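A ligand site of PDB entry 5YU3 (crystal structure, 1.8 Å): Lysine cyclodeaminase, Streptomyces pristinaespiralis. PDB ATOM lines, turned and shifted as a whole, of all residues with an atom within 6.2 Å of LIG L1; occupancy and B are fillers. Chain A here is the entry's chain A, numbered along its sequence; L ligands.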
ATOM      1  N   ARG A  49     -23.519  -0.234 -18.142  1.00  0.00           N
ATOM      2  CA  ARG A  49     -23.173   0.837 -17.231  1.00  0.00           C
ATOM      3  C   ARG A  49     -24.020   2.073 -17.524  1.00  0.00           C
ATOM      4  O   ARG A  49     -24.759   2.148 -18.522  1.00  0.00           O
ATOM      5  CB  ARG A  49     -21.684   1.170 -17.330  1.00  0.00           C
ATOM      6  CG  ARG A  49     -21.239   1.633 -18.707  1.00  0.00           C
ATOM      7  CD  ARG A  49     -19.788   2.098 -18.699  1.00  0.00           C
ATOM      8  NE  ARG A  49     -19.280   2.309 -20.053  1.00  0.00           N
ATOM      9  CZ  ARG A  49     -18.235   1.653 -20.570  1.00  0.00           C
ATOM     10  NH1 ARG A  49     -17.592   0.764 -19.844  1.00  0.00           N
ATOM     11  NH2 ARG A  49     -17.842   1.906 -21.812  1.00  0.00           N
ATOM     12  N   ILE A  61     -17.146  12.222 -19.556  1.00  0.00           N
ATOM     13  CA  ILE A  61     -18.268  11.480 -18.983  1.00  0.00           C
ATOM     14  C   ILE A  61     -17.814  10.861 -17.670  1.00  0.00           C
ATOM     15  O   ILE A  61     -16.623  10.589 -17.467  1.00  0.00           O
ATOM     16  CB  ILE A  61     -18.799  10.409 -19.974  1.00  0.00           C
ATOM     17  CG1 ILE A  61     -20.170   9.871 -19.514  1.00  0.00           C
ATOM     18  CG2 ILE A  61     -17.801   9.271 -20.197  1.00  0.00           C
ATOM     19  CD1 ILE A  61     -20.884   9.016 -20.565  1.00  0.00           C
ATOM     20  N   GLU A  63     -18.985   7.732 -15.023  1.00  0.00           N
ATOM     21  CA  GLU A  63     -19.809   6.537 -15.132  1.00  0.00           C
ATOM     22  C   GLU A  63     -19.777   5.705 -13.857  1.00  0.00           C
ATOM     23  O   GLU A  63     -18.832   5.746 -13.076  1.00  0.00           O
ATOM     24  CB  GLU A  63     -19.347   5.677 -16.321  1.00  0.00           C
ATOM     25  CG  GLU A  63     -19.519   6.380 -17.658  1.00  0.00           C
ATOM     26  CD  GLU A  63     -18.918   5.604 -18.816  1.00  0.00           C
ATOM     27  OE1 GLU A  63     -17.733   5.236 -18.748  1.00  0.00           O
ATOM     28  OE2 GLU A  63     -19.641   5.365 -19.805  1.00  0.00           O
ATOM     29  N   MET A  65     -20.388   1.563 -12.776  1.00  0.00           N
ATOM     30  CA  MET A  65     -20.283   0.228 -13.365  1.00  0.00           C
ATOM     31  C   MET A  65     -20.447  -0.820 -12.280  1.00  0.00           C
ATOM     32  O   MET A  65     -19.474  -1.197 -11.599  1.00  0.00           O
ATOM     33  CB  MET A  65     -18.942   0.065 -14.086  1.00  0.00           C
ATOM     34  CG  MET A  65     -18.663   1.183 -15.094  1.00  0.00           C
ATOM     35  SD  MET A  65     -17.030   1.147 -15.859  1.00  0.00           S
ATOM     36  CE  MET A  65     -16.956  -0.528 -16.494  1.00  0.00           C
ATOM     37  N   LYS A  77     -17.547   0.188  -9.759  1.00  0.00           N
ATOM     38  CA  LYS A  77     -16.514   1.131 -10.130  1.00  0.00           C
ATOM     39  C   LYS A  77     -17.153   2.449 -10.541  1.00  0.00           C
ATOM     40  O   LYS A  77     -18.121   2.476 -11.307  1.00  0.00           O
ATOM     41  CB  LYS A  77     -15.602   0.608 -11.254  1.00  0.00           C
ATOM     42  CG  LYS A  77     -14.511   1.644 -11.566  1.00  0.00           C
ATOM     43  CD  LYS A  77     -13.367   1.080 -12.426  1.00  0.00           C
ATOM     44  CE  LYS A  77     -13.659   1.272 -13.908  1.00  0.00           C
ATOM     45  NZ  LYS A  77     -12.632   0.587 -14.743  1.00  0.00           N
ATOM     46  N   VAL A  79     -15.946   6.007 -12.253  1.00  0.00           N
ATOM     47  CA  VAL A  79     -14.786   6.384 -13.045  1.00  0.00           C
ATOM     48  C   VAL A  79     -15.148   7.532 -13.977  1.00  0.00           C
ATOM     49  O   VAL A  79     -16.199   7.516 -14.634  1.00  0.00           O
ATOM     50  CB  VAL A  79     -14.245   5.161 -13.831  1.00  0.00           C
ATOM     51  CG1 VAL A  79     -15.362   4.506 -14.652  1.00  0.00           C
ATOM     52  CG2 VAL A  79     -13.064   5.573 -14.704  1.00  0.00           C
ATOM     53  N   GLY A  80     -14.280   8.532 -14.030  1.00  0.00           N
ATOM     54  CA  GLY A  80     -14.439   9.638 -14.942  1.00  0.00           C
ATOM     55  C   GLY A  80     -13.516   9.522 -16.143  1.00  0.00           C
ATOM     56  O   GLY A  80     -12.419   8.977 -16.062  1.00  0.00           O
ATOM     57  N   TYR A  81     -14.002  10.029 -17.280  1.00  0.00           N
ATOM     58  CA  TYR A  81     -13.194  10.271 -18.473  1.00  0.00           C
ATOM     59  C   TYR A  81     -13.184  11.779 -18.675  1.00  0.00           C
ATOM     60  O   TYR A  81     -14.240  12.374 -18.930  1.00  0.00           O
ATOM     61  CB  TYR A  81     -13.772   9.544 -19.689  1.00  0.00           C
ATOM     62  CG  TYR A  81     -13.281  10.053 -21.025  1.00  0.00           C
ATOM     63  CD1 TYR A  81     -12.029   9.702 -21.509  1.00  0.00           C
ATOM     64  CD2 TYR A  81     -14.082  10.870 -21.816  1.00  0.00           C
ATOM     65  CE1 TYR A  81     -11.575  10.163 -22.753  1.00  0.00           C
ATOM     66  CE2 TYR A  81     -13.639  11.331 -23.069  1.00  0.00           C
ATOM     67  CZ  TYR A  81     -12.380  10.967 -23.526  1.00  0.00           C
ATOM     68  OH  TYR A  81     -11.928  11.411 -24.766  1.00  0.00           O
ATOM     69  N   ILE A  94      -8.377   9.201 -17.049  1.00  0.00           N
ATOM     70  CA  ILE A  94      -9.209   8.190 -16.393  1.00  0.00           C
ATOM     71  C   ILE A  94      -8.917   8.260 -14.903  1.00  0.00           C
ATOM     72  O   ILE A  94      -7.803   7.951 -14.452  1.00  0.00           O
ATOM     73  CB  ILE A  94      -8.945   6.790 -16.959  1.00  0.00           C
ATOM     74  CG1 ILE A  94      -9.343   6.707 -18.446  1.00  0.00           C
ATOM     75  CG2 ILE A  94      -9.691   5.724 -16.127  1.00  0.00           C
ATOM     76  CD1 ILE A  94     -10.817   6.998 -18.713  1.00  0.00           C
ATOM     77  N   THR A 118      -7.720  -0.016 -13.531  1.00  0.00           N
ATOM     78  CA  THR A 118      -8.368   0.126 -14.836  1.00  0.00           C
ATOM     79  C   THR A 118      -7.348  -0.076 -15.946  1.00  0.00           C
ATOM     80  O   THR A 118      -7.599  -0.814 -16.914  1.00  0.00           O
ATOM     81  CB  THR A 118      -9.033   1.512 -14.966  1.00  0.00           C
ATOM     82  OG1 THR A 118     -10.138   1.615 -14.048  1.00  0.00           O
ATOM     83  CG2 THR A 118      -9.570   1.728 -16.408  1.00  0.00           C
ATOM     84  N   ARG A 121      -6.437  -3.954 -16.142  1.00  0.00           N
ATOM     85  CA  ARG A 121      -7.393  -4.911 -16.718  1.00  0.00           C
ATOM     86  C   ARG A 121      -7.725  -4.570 -18.165  1.00  0.00           C
ATOM     87  O   ARG A 121      -8.166  -5.457 -18.914  1.00  0.00           O
ATOM     88  CB  ARG A 121      -8.660  -5.025 -15.840  1.00  0.00           C
ATOM     89  CG  ARG A 121      -9.463  -3.755 -15.558  1.00  0.00           C
ATOM     90  CD  ARG A 121     -10.223  -3.276 -16.796  1.00  0.00           C
ATOM     91  NE  ARG A 121     -11.537  -2.717 -16.493  1.00  0.00           N
ATOM     92  CZ  ARG A 121     -12.233  -1.959 -17.333  1.00  0.00           C
ATOM     93  NH1 ARG A 121     -11.730  -1.607 -18.528  1.00  0.00           N
ATOM     94  NH2 ARG A 121     -13.442  -1.509 -16.976  1.00  0.00           N
ATOM     95  N   THR A 122      -7.520  -3.314 -18.569  1.00  0.00           N
ATOM     96  CA  THR A 122      -7.767  -2.933 -19.954  1.00  0.00           C
ATOM     97  C   THR A 122      -6.667  -3.462 -20.864  1.00  0.00           C
ATOM     98  O   THR A 122      -6.946  -3.966 -21.966  1.00  0.00           O
ATOM     99  CB  THR A 122      -7.890  -1.413 -20.052  1.00  0.00           C
ATOM    100  OG1 THR A 122      -8.920  -0.978 -19.162  1.00  0.00           O
ATOM    101  CG2 THR A 122      -8.253  -0.964 -21.473  1.00  0.00           C
ATOM    102  N   ALA A 235     -13.143   4.567 -25.968  1.00  0.00           N
ATOM    103  CA  ALA A 235     -14.559   4.409 -25.626  1.00  0.00           C
ATOM    104  C   ALA A 235     -14.910   5.412 -24.542  1.00  0.00           C
ATOM    105  O   ALA A 235     -14.246   5.442 -23.506  1.00  0.00           O
ATOM    106  CB  ALA A 235     -14.874   2.986 -25.117  1.00  0.00           C
ATOM    107  N   ASP A 236     -15.933   6.229 -24.783  1.00  0.00           N
ATOM    108  CA  ASP A 236     -16.418   7.156 -23.762  1.00  0.00           C
ATOM    109  C   ASP A 236     -17.809   7.669 -24.100  1.00  0.00           C
ATOM    110  O   ASP A 236     -18.799   7.166 -23.570  1.00  0.00           O
ATOM    111  CB  ASP A 236     -15.418   8.301 -23.581  1.00  0.00           C
ATOM    112  CG  ASP A 236     -14.914   8.897 -24.904  1.00  0.00           C
ATOM    113  OD1 ASP A 236     -13.698   8.773 -25.189  1.00  0.00           O
ATOM    114  OD2 ASP A 236     -15.713   9.520 -25.626  1.00  0.00           O
ATOM    115  N   THR A 302     -14.923  -2.049 -24.662  1.00  0.00           N
ATOM    116  CA  THR A 302     -15.567  -0.945 -23.968  1.00  0.00           C
ATOM    117  C   THR A 302     -15.321  -0.980 -22.467  1.00  0.00           C
ATOM    118  O   THR A 302     -15.487   0.064 -21.823  1.00  0.00           O
ATOM    119  CB  THR A 302     -17.088  -0.956 -24.213  1.00  0.00           C
ATOM    120  OG1 THR A 302     -17.657  -2.163 -23.673  1.00  0.00           O
ATOM    121  CG2 THR A 302     -17.373  -0.865 -25.711  1.00  0.00           C
ATOM    122  N   GLY A 303     -14.920  -2.125 -21.923  1.00  0.00           N
ATOM    123  CA  GLY A 303     -14.724  -2.293 -20.491  1.00  0.00           C
ATOM    124  C   GLY A 303     -16.033  -2.634 -19.809  1.00  0.00           C
ATOM    125  O   GLY A 303     -17.072  -2.038 -20.137  1.00  0.00           O
ATOM    126  N   PHE A 304     -16.027  -3.597 -18.897  1.00  0.00           N
ATOM    127  CA  PHE A 304     -17.240  -3.832 -18.150  1.00  0.00           C
ATOM    128  C   PHE A 304     -16.871  -4.273 -16.739  1.00  0.00           C
ATOM    129  O   PHE A 304     -15.755  -4.721 -16.469  1.00  0.00           O
ATOM    130  CB  PHE A 304     -18.201  -4.820 -18.865  1.00  0.00           C
ATOM    131  CG  PHE A 304     -17.666  -6.216 -19.066  1.00  0.00           C
ATOM    132  CD1 PHE A 304     -16.683  -6.484 -20.035  1.00  0.00           C
ATOM    133  CD2 PHE A 304     -18.193  -7.285 -18.348  1.00  0.00           C
ATOM    134  CE1 PHE A 304     -16.225  -7.773 -20.242  1.00  0.00           C
ATOM    135  CE2 PHE A 304     -17.730  -8.586 -18.551  1.00  0.00           C
ATOM    136  CZ  PHE A 304     -16.746  -8.830 -19.498  1.00  0.00           C
ATOM    137  N   GLU A 307     -14.728  -7.144 -15.239  1.00  0.00           N
ATOM    138  CA  GLU A 307     -13.275  -7.067 -15.320  1.00  0.00           C
ATOM    139  C   GLU A 307     -12.702  -6.353 -14.108  1.00  0.00           C
ATOM    140  O   GLU A 307     -11.646  -6.739 -13.595  1.00  0.00           O
ATOM    141  CB  GLU A 307     -12.849  -6.357 -16.599  1.00  0.00           C
ATOM    142  CG  GLU A 307     -13.387  -7.015 -17.876  1.00  0.00           C
ATOM    143  CD  GLU A 307     -13.077  -6.210 -19.133  1.00  0.00           C
ATOM    144  OE1 GLU A 307     -13.001  -4.969 -19.056  1.00  0.00           O
ATOM    145  OE2 GLU A 307     -12.900  -6.830 -20.212  1.00  0.00           O
ATOM    146  N   ASP A 308     -13.375  -5.291 -13.654  1.00  0.00           N
ATOM    147  CA  ASP A 308     -12.916  -4.558 -12.478  1.00  0.00           C
ATOM    148  C   ASP A 308     -13.049  -5.399 -11.213  1.00  0.00           C
ATOM    149  O   ASP A 308     -12.184  -5.343 -10.331  1.00  0.00           O
ATOM    150  CB  ASP A 308     -13.697  -3.264 -12.363  1.00  0.00           C
ATOM    151  CG  ASP A 308     -13.554  -2.415 -13.593  1.00  0.00           C
ATOM    152  OD1 ASP A 308     -12.408  -1.983 -13.849  1.00  0.00           O
ATOM    153  OD2 ASP A 308     -14.553  -2.190 -14.313  1.00  0.00           O
HETATM  154  N1  LIG L   1     -14.583   2.996 -20.178  1.00  0.00           N
HETATM  155  C1  LIG L   1     -13.678   3.048 -18.909  1.00  0.00           C
HETATM  156  C2  LIG L   1     -13.856   1.754 -18.072  1.00  0.00           C
HETATM  157  O1  LIG L   1     -13.441   1.871 -16.896  1.00  0.00           O
HETATM  158  C3  LIG L   1     -14.068   4.106 -18.315  1.00  0.00           C
HETATM  159  C4  LIG L   1     -14.394   5.122 -19.539  1.00  0.00           C
HETATM  160  C5  LIG L   1     -14.448   4.404 -20.615  1.00  0.00           C
HETATM  161  O2  LIG L   1     -14.338   0.660 -18.516  1.00  0.00           O
HETATM  162  P1  LG2 L   2      -5.147   9.678 -22.197  1.00  0.00           P
HETATM  163  O1  LG2 L   2      -5.684  11.076 -22.167  1.00  0.00           O
HETATM  164  O2  LG2 L   2      -4.067   9.266 -21.211  1.00  0.00           O
HETATM  165  O3  LG2 L   2      -4.527   9.415 -23.660  1.00  0.00           O
HETATM  166  C1  LG2 L   2      -5.334   9.625 -24.825  1.00  0.00           C
HETATM  167  C2  LG2 L   2      -4.373  10.061 -25.929  1.00  0.00           C
HETATM  168  O4  LG2 L   2      -5.087  10.121 -27.170  1.00  0.00           O
HETATM  169  C3  LG2 L   2      -3.835  11.479 -25.683  1.00  0.00           C
HETATM  170  O5  LG2 L   2      -2.396  11.452 -25.603  1.00  0.00           O
HETATM  171  C4  LG2 L   2      -4.310  12.263 -26.889  1.00  0.00           C
HETATM  172  O6  LG2 L   2      -3.380  13.239 -27.351  1.00  0.00           O
HETATM  173  C5  LG2 L   2      -4.484  11.170 -27.921  1.00  0.00           C
HETATM  174  N1  LG2 L   2      -5.364  11.478 -29.075  1.00  0.00           N
HETATM  175  C6  LG2 L   2      -6.502  12.219 -29.097  1.00  0.00           C
HETATM  176  N2  LG2 L   2      -7.024  12.233 -30.363  1.00  0.00           N
HETATM  177  C7  LG2 L   2      -6.212  11.491 -31.146  1.00  0.00           C
HETATM  178  C8  LG2 L   2      -6.147  11.087 -32.560  1.00  0.00           C
HETATM  179  N3  LG2 L   2      -7.106  11.476 -33.434  1.00  0.00           N
HETATM  180  N4  LG2 L   2      -5.129  10.284 -32.942  1.00  0.00           N
HETATM  181  C9  LG2 L   2      -4.157   9.864 -32.110  1.00  0.00           C
HETATM  182  N5  LG2 L   2      -4.143  10.208 -30.806  1.00  0.00           N
HETATM  183  C10 LG2 L   2      -5.120  10.995 -30.283  1.00  0.00           C
HETATM  184  O7  LG2 L   2      -6.417   8.685 -22.051  1.00  0.00           O
HETATM  185  P2  LG2 L   2      -6.385   7.097 -21.830  1.00  0.00           P
HETATM  186  O8  LG2 L   2      -5.211   6.529 -22.598  1.00  0.00           O
HETATM  187  O9  LG2 L   2      -6.537   6.824 -20.351  1.00  0.00           O
HETATM  188  O10 LG2 L   2      -7.771   6.630 -22.526  1.00  0.00           O
HETATM  189  C11 LG2 L   2      -7.881   6.590 -23.944  1.00  0.00           C
HETATM  190  C12 LG2 L   2      -9.258   6.041 -24.314  1.00  0.00           C
HETATM  191  O11 LG2 L   2      -9.427   4.735 -23.760  1.00  0.00           O
HETATM  192  C13 LG2 L   2     -10.383   6.880 -23.744  1.00  0.00           C
HETATM  193  O12 LG2 L   2     -11.475   6.903 -24.702  1.00  0.00           O
HETATM  194  C14 LG2 L   2     -10.835   6.081 -22.544  1.00  0.00           C
HETATM  195  O13 LG2 L   2     -12.176   6.400 -22.117  1.00  0.00           O
HETATM  196  C15 LG2 L   2     -10.681   4.679 -23.088  1.00  0.00           C
HETATM  197  N6  LG2 L   2     -10.652   3.618 -22.081  1.00  0.00           N
HETATM  198  C16 LG2 L   2     -11.178   2.426 -22.419  1.00  0.00           C
HETATM  199  C17 LG2 L   2     -11.197   1.380 -21.515  1.00  0.00           C
HETATM  200  C18 LG2 L   2     -11.771   0.073 -21.949  1.00  0.00           C
HETATM  201  O14 LG2 L   2     -12.001  -0.794 -21.126  1.00  0.00           O
HETATM  202  N7  LG2 L   2     -11.968  -0.137 -23.260  1.00  0.00           N
HETATM  203  C19 LG2 L   2     -10.617   1.538 -20.256  1.00  0.00           C
HETATM  204  C20 LG2 L   2     -10.058   2.772 -19.942  1.00  0.00           C
HETATM  205  C21 LG2 L   2     -10.081   3.808 -20.883  1.00  0.00           C
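Merely in contact with LIG L1: Glu 63 (3.4 Å), Met 65 (3.5 Å), Val 79 (3.9 Å), Thr 118 (3.9 Å), Ala 235 (3.1 Å) and Gly 303 (3.6 Å). Within 4 Å of LIG L1: Arg 49, Glu 63, Met 65, Lys 77, Val 79, Thr 118, Arg 121, Ala 235, Thr 302 and Gly 303. The nearest printed residue that does not touch LIG L1 is Ile 94 (4.1 Å).
The side-chain amino group (NZ) of Lys 77 is in salt-bridge range of an oxygen (O1) of LIG L1. NH2 of Arg 121 lies within salt-bridge range of O2 of LIG L1, 2.8 Å away. N1 of LIG L1 lies within hydrogen-bond range of O of Thr 302. O2 of LIG L1 lies within salt-bridge range of NH1 of Arg 49 (3.5 Å). The guanidinium group (NH1) of Arg 121 sits at hydrogen-bond distance from an oxygen (O14) of LG2 L2. O12 of LG2 L2 sits at hydrogen-bond distance from N of Ala 235, at 3.1 Å. An oxygen (O13) of LG2 L2 is in hydrogen-bond range of the backbone carbonyl oxygen (O) of Ala 235 (2.7 Å). The backbone NH (N) of Gly 303 sits close to an oxygen (O14) of LG2 L2 (3.3 Å). O12 of LG2 L2 lies within hydrogen-bond range of OD1 of Asp 236 (2.9 Å).
The side-chain amino group (NZ) of Lys 77 sits at hydrogen-bond distance from the side-chain hydroxyl (OG1) of Thr 118 (2.8 Å). The side-chain carboxylate (OD1) of Asp 308 lies within salt-bridge range of the side-chain amino group (NZ) of Lys 77, at 2.7 Å. NE of Arg 121 is in salt-bridge range of OD1 of Asp 308, at 2.9 Å. The guanidinium group of Arg 121 is in hydrogen-bond range of the side-chain hydroxyl of Thr 122. The guanidinium group (NH1) of Arg 121 is in salt-bridge range of the side-chain carboxylate (OE1) of Glu 307, 3.6 Å away. The side-chain carboxylate (OE2) of Glu 63 lies within salt-bridge range of the guanidinium group (NE) of Arg 49 (3.1 Å). N of Glu 63 lies within hydrogen-bond range of O of Val 79 (2.8 Å). The guanidinium group (NH1) of Arg 49 sits at hydrogen-bond distance from the backbone carbonyl oxygen (O) of Gly 303, 2.9 Å away.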
